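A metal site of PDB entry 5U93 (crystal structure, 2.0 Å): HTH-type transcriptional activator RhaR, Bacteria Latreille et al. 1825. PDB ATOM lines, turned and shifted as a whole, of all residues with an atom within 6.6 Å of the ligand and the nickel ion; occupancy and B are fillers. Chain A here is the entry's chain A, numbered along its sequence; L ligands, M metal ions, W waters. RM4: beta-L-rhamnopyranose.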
ATOM      1  N   LEU A   7     -31.400 -27.472  26.435  1.00  0.00           N
ATOM      2  CA  LEU A   7     -30.571 -27.694  27.608  1.00  0.00           C
ATOM      3  C   LEU A   7     -31.366 -28.308  28.755  1.00  0.00           C
ATOM      4  O   LEU A   7     -32.510 -27.913  29.022  1.00  0.00           O
ATOM      5  CB  LEU A   7     -29.952 -26.374  28.047  1.00  0.00           C
ATOM      6  CG  LEU A   7     -29.176 -25.644  26.959  1.00  0.00           C
ATOM      7  CD1 LEU A   7     -28.512 -24.424  27.585  1.00  0.00           C
ATOM      8  CD2 LEU A   7     -28.148 -26.545  26.293  1.00  0.00           C
ATOM      9  N   PHE A  12     -27.167 -29.258  34.225  1.00  0.00           N
ATOM     10  CA  PHE A  12     -26.797 -27.947  34.721  1.00  0.00           C
ATOM     11  C   PHE A  12     -26.971 -27.749  36.234  1.00  0.00           C
ATOM     12  O   PHE A  12     -26.413 -26.808  36.786  1.00  0.00           O
ATOM     13  CB  PHE A  12     -27.507 -26.826  33.927  1.00  0.00           C
ATOM     14  CG  PHE A  12     -26.945 -26.627  32.558  1.00  0.00           C
ATOM     15  CD1 PHE A  12     -25.944 -25.693  32.337  1.00  0.00           C
ATOM     16  CD2 PHE A  12     -27.357 -27.425  31.501  1.00  0.00           C
ATOM     17  CE1 PHE A  12     -25.376 -25.546  31.068  1.00  0.00           C
ATOM     18  CE2 PHE A  12     -26.797 -27.289  30.229  1.00  0.00           C
ATOM     19  CZ  PHE A  12     -25.810 -26.337  30.011  1.00  0.00           C
ATOM     20  N   ALA A  23     -24.610 -19.883  36.857  1.00  0.00           N
ATOM     21  CA  ALA A  23     -23.704 -20.191  35.781  1.00  0.00           C
ATOM     22  C   ALA A  23     -23.025 -18.906  35.299  1.00  0.00           C
ATOM     23  O   ALA A  23     -23.667 -18.054  34.656  1.00  0.00           O
ATOM     24  CB  ALA A  23     -24.455 -20.850  34.646  1.00  0.00           C
ATOM     25  N   ARG A  25     -20.718 -16.590  33.020  1.00  0.00           N
ATOM     26  CA  ARG A  25     -20.240 -16.514  31.649  1.00  0.00           C
ATOM     27  C   ARG A  25     -19.256 -15.354  31.545  1.00  0.00           C
ATOM     28  O   ARG A  25     -19.654 -14.203  31.293  1.00  0.00           O
ATOM     29  CB  ARG A  25     -21.427 -16.354  30.699  1.00  0.00           C
ATOM     30  CG  ARG A  25     -22.442 -17.507  30.793  1.00  0.00           C
ATOM     31  CD  ARG A  25     -21.807 -18.820  30.285  1.00  0.00           C
ATOM     32  NE  ARG A  25     -22.690 -19.984  30.390  1.00  0.00           N
ATOM     33  CZ  ARG A  25     -22.616 -20.907  31.353  1.00  0.00           C
ATOM     34  NH1 ARG A  25     -21.708 -20.803  32.309  1.00  0.00           N
ATOM     35  NH2 ARG A  25     -23.452 -21.940  31.353  1.00  0.00           N
ATOM     36  N   GLN A  28     -19.458 -14.529  27.966  1.00  0.00           N
ATOM     37  CA  GLN A  28     -20.404 -15.324  27.180  1.00  0.00           C
ATOM     38  C   GLN A  28     -19.953 -15.283  25.727  1.00  0.00           C
ATOM     39  O   GLN A  28     -19.868 -14.214  25.122  1.00  0.00           O
ATOM     40  CB  GLN A  28     -21.814 -14.747  27.294  1.00  0.00           C
ATOM     41  CG  GLN A  28     -22.849 -15.407  26.382  1.00  0.00           C
ATOM     42  CD  GLN A  28     -23.236 -16.806  26.861  1.00  0.00           C
ATOM     43  OE1 GLN A  28     -23.843 -16.971  27.926  1.00  0.00           O
ATOM     44  NE2 GLN A  28     -22.870 -17.811  26.071  1.00  0.00           N
ATOM     45  N   ASP A  29     -19.650 -16.452  25.173  1.00  0.00           N
ATOM     46  CA  ASP A  29     -19.303 -16.539  23.764  1.00  0.00           C
ATOM     47  C   ASP A  29     -20.574 -16.728  22.948  1.00  0.00           C
ATOM     48  O   ASP A  29     -21.678 -16.812  23.502  1.00  0.00           O
ATOM     49  CB  ASP A  29     -18.339 -17.707  23.534  1.00  0.00           C
ATOM     50  CG  ASP A  29     -17.104 -17.615  24.428  1.00  0.00           C
ATOM     51  OD1 ASP A  29     -16.220 -16.776  24.128  1.00  0.00           O
ATOM     52  OD2 ASP A  29     -17.006 -18.383  25.411  1.00  0.00           O
ATOM     53  N   PHE A  31     -23.448 -18.433  21.190  1.00  0.00           N
ATOM     54  CA  PHE A  31     -24.139 -19.608  21.696  1.00  0.00           C
ATOM     55  C   PHE A  31     -25.399 -19.866  20.878  1.00  0.00           C
ATOM     56  O   PHE A  31     -26.210 -18.965  20.671  1.00  0.00           O
ATOM     57  CB  PHE A  31     -24.481 -19.451  23.180  1.00  0.00           C
ATOM     58  CG  PHE A  31     -24.837 -20.753  23.844  1.00  0.00           C
ATOM     59  CD1 PHE A  31     -26.161 -21.143  23.956  1.00  0.00           C
ATOM     60  CD2 PHE A  31     -23.851 -21.584  24.335  1.00  0.00           C
ATOM     61  CE1 PHE A  31     -26.480 -22.354  24.571  1.00  0.00           C
ATOM     62  CE2 PHE A  31     -24.166 -22.795  24.936  1.00  0.00           C
ATOM     63  CZ  PHE A  31     -25.482 -23.174  25.051  1.00  0.00           C
ATOM     64  N   HIS A  34     -31.401 -22.085  21.449  1.00  0.00           N
ATOM     65  CA  HIS A  34     -31.739 -23.225  22.294  1.00  0.00           C
ATOM     66  C   HIS A  34     -32.935 -22.924  23.184  1.00  0.00           C
ATOM     67  O   HIS A  34     -33.249 -21.761  23.468  1.00  0.00           O
ATOM     68  CB  HIS A  34     -30.553 -23.593  23.181  1.00  0.00           C
ATOM     69  CG  HIS A  34     -30.218 -22.538  24.173  1.00  0.00           C
ATOM     70  ND1 HIS A  34     -29.464 -21.423  23.857  1.00  0.00           N
ATOM     71  CD2 HIS A  34     -30.579 -22.381  25.472  1.00  0.00           C
ATOM     72  CE1 HIS A  34     -29.370 -20.642  24.919  1.00  0.00           C
ATOM     73  NE2 HIS A  34     -30.032 -21.204  25.906  1.00  0.00           N
ATOM     74  N   THR A  35     -33.584 -23.985  23.635  1.00  0.00           N
ATOM     75  CA  THR A  35     -34.563 -23.881  24.713  1.00  0.00           C
ATOM     76  C   THR A  35     -34.003 -24.630  25.906  1.00  0.00           C
ATOM     77  O   THR A  35     -32.834 -25.060  25.885  1.00  0.00           O
ATOM     78  CB  THR A  35     -35.908 -24.504  24.318  1.00  0.00           C
ATOM     79  OG1 THR A  35     -35.704 -25.860  23.899  1.00  0.00           O
ATOM     80  CG2 THR A  35     -36.532 -23.724  23.156  1.00  0.00           C
ATOM     81  N   HIS A  36     -34.822 -24.810  26.935  1.00  0.00           N
ATOM     82  CA  HIS A  36     -34.392 -25.393  28.204  1.00  0.00           C
ATOM     83  C   HIS A  36     -35.540 -26.204  28.777  1.00  0.00           C
ATOM     84  O   HIS A  36     -36.661 -26.119  28.293  1.00  0.00           O
ATOM     85  CB  HIS A  36     -34.052 -24.298  29.241  1.00  0.00           C
ATOM     86  CG  HIS A  36     -33.463 -23.039  28.687  1.00  0.00           C
ATOM     87  ND1 HIS A  36     -34.200 -22.119  27.970  1.00  0.00           N
ATOM     88  CD2 HIS A  36     -32.220 -22.505  28.807  1.00  0.00           C
ATOM     89  CE1 HIS A  36     -33.438 -21.097  27.643  1.00  0.00           C
ATOM     90  NE2 HIS A  36     -32.225 -21.312  28.136  1.00  0.00           N
ATOM     91  N   PHE A  38     -35.539 -25.740  32.156  1.00  0.00           N
ATOM     92  CA  PHE A  38     -35.442 -24.953  33.388  1.00  0.00           C
ATOM     93  C   PHE A  38     -35.574 -23.494  32.985  1.00  0.00           C
ATOM     94  O   PHE A  38     -35.445 -23.186  31.798  1.00  0.00           O
ATOM     95  CB  PHE A  38     -34.105 -25.195  34.120  1.00  0.00           C
ATOM     96  CG  PHE A  38     -32.882 -25.029  33.239  1.00  0.00           C
ATOM     97  CD1 PHE A  38     -32.254 -23.775  33.120  1.00  0.00           C
ATOM     98  CD2 PHE A  38     -32.334 -26.120  32.567  1.00  0.00           C
ATOM     99  CE1 PHE A  38     -31.110 -23.629  32.311  1.00  0.00           C
ATOM    100  CE2 PHE A  38     -31.193 -25.980  31.751  1.00  0.00           C
ATOM    101  CZ  PHE A  38     -30.585 -24.720  31.632  1.00  0.00           C
ATOM    102  N   GLU A  40     -34.395 -19.224  33.620  1.00  0.00           N
ATOM    103  CA  GLU A  40     -33.184 -18.504  34.016  1.00  0.00           C
ATOM    104  C   GLU A  40     -33.346 -16.990  34.046  1.00  0.00           C
ATOM    105  O   GLU A  40     -34.132 -16.427  33.296  1.00  0.00           O
ATOM    106  CB  GLU A  40     -31.986 -18.903  33.121  1.00  0.00           C
ATOM    107  CG  GLU A  40     -32.188 -18.578  31.654  1.00  0.00           C
ATOM    108  CD  GLU A  40     -31.162 -19.231  30.746  1.00  0.00           C
ATOM    109  OE1 GLU A  40     -30.571 -20.285  31.095  1.00  0.00           O
ATOM    110  OE2 GLU A  40     -30.943 -18.671  29.658  1.00  0.00           O
ATOM    111  N   VAL A  42     -31.023 -13.609  33.563  1.00  0.00           N
ATOM    112  CA  VAL A  42     -29.758 -13.195  32.958  1.00  0.00           C
ATOM    113  C   VAL A  42     -29.454 -11.772  33.402  1.00  0.00           C
ATOM    114  O   VAL A  42     -30.301 -10.875  33.257  1.00  0.00           O
ATOM    115  CB  VAL A  42     -29.855 -13.192  31.432  1.00  0.00           C
ATOM    116  CG1 VAL A  42     -28.523 -12.815  30.811  1.00  0.00           C
ATOM    117  CG2 VAL A  42     -30.384 -14.562  30.917  1.00  0.00           C
ATOM    118  N   HIS A  51     -28.427 -10.353  21.908  1.00  0.00           N
ATOM    119  CA  HIS A  51     -29.246 -11.401  22.468  1.00  0.00           C
ATOM    120  C   HIS A  51     -30.514 -11.515  21.623  1.00  0.00           C
ATOM    121  O   HIS A  51     -31.310 -10.568  21.568  1.00  0.00           O
ATOM    122  CB  HIS A  51     -29.597 -11.071  23.917  1.00  0.00           C
ATOM    123  CG  HIS A  51     -30.501 -12.070  24.576  1.00  0.00           C
ATOM    124  ND1 HIS A  51     -31.415 -11.715  25.545  1.00  0.00           N
ATOM    125  CD2 HIS A  51     -30.603 -13.413  24.439  1.00  0.00           C
ATOM    126  CE1 HIS A  51     -32.058 -12.799  25.961  1.00  0.00           C
ATOM    127  NE2 HIS A  51     -31.577 -13.836  25.305  1.00  0.00           N
ATOM    128  N   ILE A  68     -36.121 -15.259  31.518  1.00  0.00           N
ATOM    129  CA  ILE A  68     -36.256 -16.269  30.469  1.00  0.00           C
ATOM    130  C   ILE A  68     -37.042 -17.464  30.976  1.00  0.00           C
ATOM    131  O   ILE A  68     -36.757 -17.995  32.043  1.00  0.00           O
ATOM    132  CB  ILE A  68     -34.872 -16.795  30.034  1.00  0.00           C
ATOM    133  CG1 ILE A  68     -33.904 -15.635  29.733  1.00  0.00           C
ATOM    134  CG2 ILE A  68     -34.996 -17.737  28.832  1.00  0.00           C
ATOM    135  CD1 ILE A  68     -34.280 -14.806  28.537  1.00  0.00           C
ATOM    136  N   ASP A  72     -38.678 -20.480  26.075  1.00  0.00           N
ATOM    137  CA  ASP A  72     -38.146 -19.411  25.232  1.00  0.00           C
ATOM    138  C   ASP A  72     -36.966 -19.971  24.445  1.00  0.00           C
ATOM    139  O   ASP A  72     -36.140 -20.703  24.981  1.00  0.00           O
ATOM    140  CB  ASP A  72     -37.664 -18.229  26.083  1.00  0.00           C
ATOM    141  CG  ASP A  72     -38.805 -17.446  26.685  1.00  0.00           C
ATOM    142  OD1 ASP A  72     -39.924 -17.454  26.129  1.00  0.00           O
ATOM    143  OD2 ASP A  72     -38.583 -16.808  27.730  1.00  0.00           O
ATOM    144  N   HIS A  74     -33.580 -18.859  22.550  1.00  0.00           N
ATOM    145  CA  HIS A  74     -32.698 -17.689  22.503  1.00  0.00           C
ATOM    146  C   HIS A  74     -31.263 -18.060  22.208  1.00  0.00           C
ATOM    147  O   HIS A  74     -30.879 -19.241  22.272  1.00  0.00           O
ATOM    148  CB  HIS A  74     -32.831 -16.813  23.767  1.00  0.00           C
ATOM    149  CG  HIS A  74     -32.267 -17.417  25.019  1.00  0.00           C
ATOM    150  ND1 HIS A  74     -31.900 -16.664  26.107  1.00  0.00           N
ATOM    151  CD2 HIS A  74     -32.009 -18.714  25.349  1.00  0.00           C
ATOM    152  CE1 HIS A  74     -31.447 -17.462  27.060  1.00  0.00           C
ATOM    153  NE2 HIS A  74     -31.496 -18.710  26.627  1.00  0.00           N
ATOM    154  N   SER A  75     -30.484 -17.044  21.858  1.00  0.00           N
ATOM    155  CA  SER A  75     -29.106 -17.222  21.438  1.00  0.00           C
ATOM    156  C   SER A  75     -28.294 -15.957  21.679  1.00  0.00           C
ATOM    157  O   SER A  75     -28.837 -14.879  21.893  1.00  0.00           O
ATOM    158  CB  SER A  75     -29.048 -17.589  19.951  1.00  0.00           C
ATOM    159  OG  SER A  75     -29.485 -16.507  19.154  1.00  0.00           O
ATOM    160  N   TYR A  76     -26.969 -16.103  21.627  1.00  0.00           N
ATOM    161  CA  TYR A  76     -26.062 -14.986  21.738  1.00  0.00           C
ATOM    162  C   TYR A  76     -25.161 -14.965  20.514  1.00  0.00           C
ATOM    163  O   TYR A  76     -24.590 -15.981  20.160  1.00  0.00           O
ATOM    164  CB  TYR A  76     -25.224 -15.109  23.001  1.00  0.00           C
ATOM    165  CG  TYR A  76     -26.067 -15.004  24.233  1.00  0.00           C
ATOM    166  CD1 TYR A  76     -26.489 -16.142  24.896  1.00  0.00           C
ATOM    167  CD2 TYR A  76     -26.480 -13.774  24.707  1.00  0.00           C
ATOM    168  CE1 TYR A  76     -27.287 -16.051  26.039  1.00  0.00           C
ATOM    169  CE2 TYR A  76     -27.274 -13.666  25.836  1.00  0.00           C
ATOM    170  CZ  TYR A  76     -27.677 -14.816  26.491  1.00  0.00           C
ATOM    171  OH  TYR A  76     -28.479 -14.736  27.617  1.00  0.00           O
ATOM    172  N   LEU A  84     -21.688 -11.915  31.676  1.00  0.00           N
ATOM    173  CA  LEU A  84     -23.011 -12.061  32.266  1.00  0.00           C
ATOM    174  C   LEU A  84     -23.070 -13.234  33.228  1.00  0.00           C
ATOM    175  O   LEU A  84     -22.125 -14.007  33.334  1.00  0.00           O
ATOM    176  CB  LEU A  84     -24.095 -12.177  31.174  1.00  0.00           C
ATOM    177  CG  LEU A  84     -24.110 -13.347  30.172  1.00  0.00           C
ATOM    178  CD1 LEU A  84     -24.700 -14.600  30.785  1.00  0.00           C
ATOM    179  CD2 LEU A  84     -24.890 -12.960  28.931  1.00  0.00           C
ATOM    180  N   ASN A  86     -25.955 -16.291  34.450  1.00  0.00           N
ATOM    181  CA  ASN A  86     -27.271 -16.902  34.404  1.00  0.00           C
ATOM    182  C   ASN A  86     -27.591 -17.439  35.780  1.00  0.00           C
ATOM    183  O   ASN A  86     -26.852 -18.244  36.326  1.00  0.00           O
ATOM    184  CB  ASN A  86     -27.314 -18.071  33.409  1.00  0.00           C
ATOM    185  CG  ASN A  86     -27.073 -17.635  31.989  1.00  0.00           C
ATOM    186  OD1 ASN A  86     -27.793 -16.802  31.455  1.00  0.00           O
ATOM    187  ND2 ASN A  86     -26.054 -18.217  31.359  1.00  0.00           N
ATOM    188  N   ILE A  88     -29.958 -19.839  37.064  1.00  0.00           N
ATOM    189  CA  ILE A  88     -30.882 -20.847  36.539  1.00  0.00           C
ATOM    190  C   ILE A  88     -31.675 -21.455  37.694  1.00  0.00           C
ATOM    191  O   ILE A  88     -31.165 -21.625  38.796  1.00  0.00           O
ATOM    192  CB  ILE A  88     -30.133 -21.923  35.730  1.00  0.00           C
ATOM    193  CG1 ILE A  88     -29.143 -22.689  36.613  1.00  0.00           C
ATOM    194  CG2 ILE A  88     -29.377 -21.268  34.563  1.00  0.00           C
ATOM    195  CD1 ILE A  88     -28.429 -23.845  35.883  1.00  0.00           C
HETATM  196  C1  RM4 L   1     -25.411 -20.911  28.120  1.00  0.00           C
HETATM  197  C2  RM4 L   1     -26.285 -19.784  27.689  1.00  0.00           C
HETATM  198  C3  RM4 L   1     -27.705 -20.136  27.823  1.00  0.00           C
HETATM  199  C4  RM4 L   1     -28.080 -20.666  29.143  1.00  0.00           C
HETATM  200  C5  RM4 L   1     -27.147 -21.761  29.599  1.00  0.00           C
HETATM  201  C6  RM4 L   1     -27.383 -22.059  31.019  1.00  0.00           C
HETATM  202  O1  RM4 L   1     -24.125 -20.548  28.100  1.00  0.00           O
HETATM  203  O2  RM4 L   1     -25.985 -18.619  28.447  1.00  0.00           O
HETATM  204  O3  RM4 L   1     -28.547 -19.009  27.536  1.00  0.00           O
HETATM  205  O4  RM4 L   1     -29.422 -21.115  29.088  1.00  0.00           O
HETATM  206  O5  RM4 L   1     -25.763 -21.384  29.469  1.00  0.00           O
HETATM  207 NI    NI M   1     -30.559 -20.039  27.754  1.00  0.00          NI
HETATM  208  O   HOH W   1     -23.253 -23.461  28.461  1.00  0.00           O
HETATM  209  O   HOH W   2     -28.810 -16.966  29.059  1.00  0.00           O
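An oxygen (O2) of the ligand sits at hydrogen-bond distance from the side-chain amide oxygen (OE1) of Gln 28 (2.8 Å). NE of Arg 25 is in hydrogen-bond range of O1 of the ligand (2.8 Å). An oxygen (O2) of the ligand is in hydrogen-bond range of the side-chain amide nitrogen (ND2) of Asn 86.
A ring nitrogen (NE2) of His 51 sits at hydrogen-bond distance from a ring nitrogen (ND1) of His 74 (3.0 Å). N of Ile 68 is in hydrogen-bond range of O of Glu 40, at 2.9 Å. N of Arg 25 is in hydrogen-bond range of O of Leu 84 (3.0 Å). O of Asn 86 is in hydrogen-bond range of N of Ala 23 (2.8 Å). The backbone carbonyl oxygen (O) of Tyr 76 lies within hydrogen-bond range of the backbone NH (N) of Phe 31, at 2.9 Å. O of Thr 35 lies within hydrogen-bond range of N of Leu 7.
Leu 7 touches the ligand. Phe 31 touches the ligand (CZ to C1, 3.8 Å). Tyr 76 touches the ligand. Hydrophobic or aromatic side chains within 4 Å of the ligand: Leu 7, Phe 31, His 34, His 36, His 74 and Tyr 76. Of the 22 residues printed, 10 come within 4 Å of the ligand.
The nearest printed residue that does not touch the nickel ion is Leu 7 (4.8 Å).
NE2 of His 74 binds the nickel ion, at 2.0 Å. O4 of the ligand binds the nickel ion (2.1 Å). NE2 of His 36 binds the nickel ion, at 2.1 Å. NE2 of His 34 binds the nickel ion. An oxygen (O3) of the ligand is bound to the nickel ion. The nickel ion is bound by OE2 of Glu 40, at 2.4 Å. The nickel ion has six donor atoms within binding distance.
Water W2 lies within hydrogen-bond range of OD1 of Asn 86, OH of Tyr 76 and O2 of the ligand. Water W1 lies within hydrogen-bond range of an oxygen (O1) of the ligand (3.1 Å) and the guanidinium group (NH2) of Arg 25 (3.3 Å).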
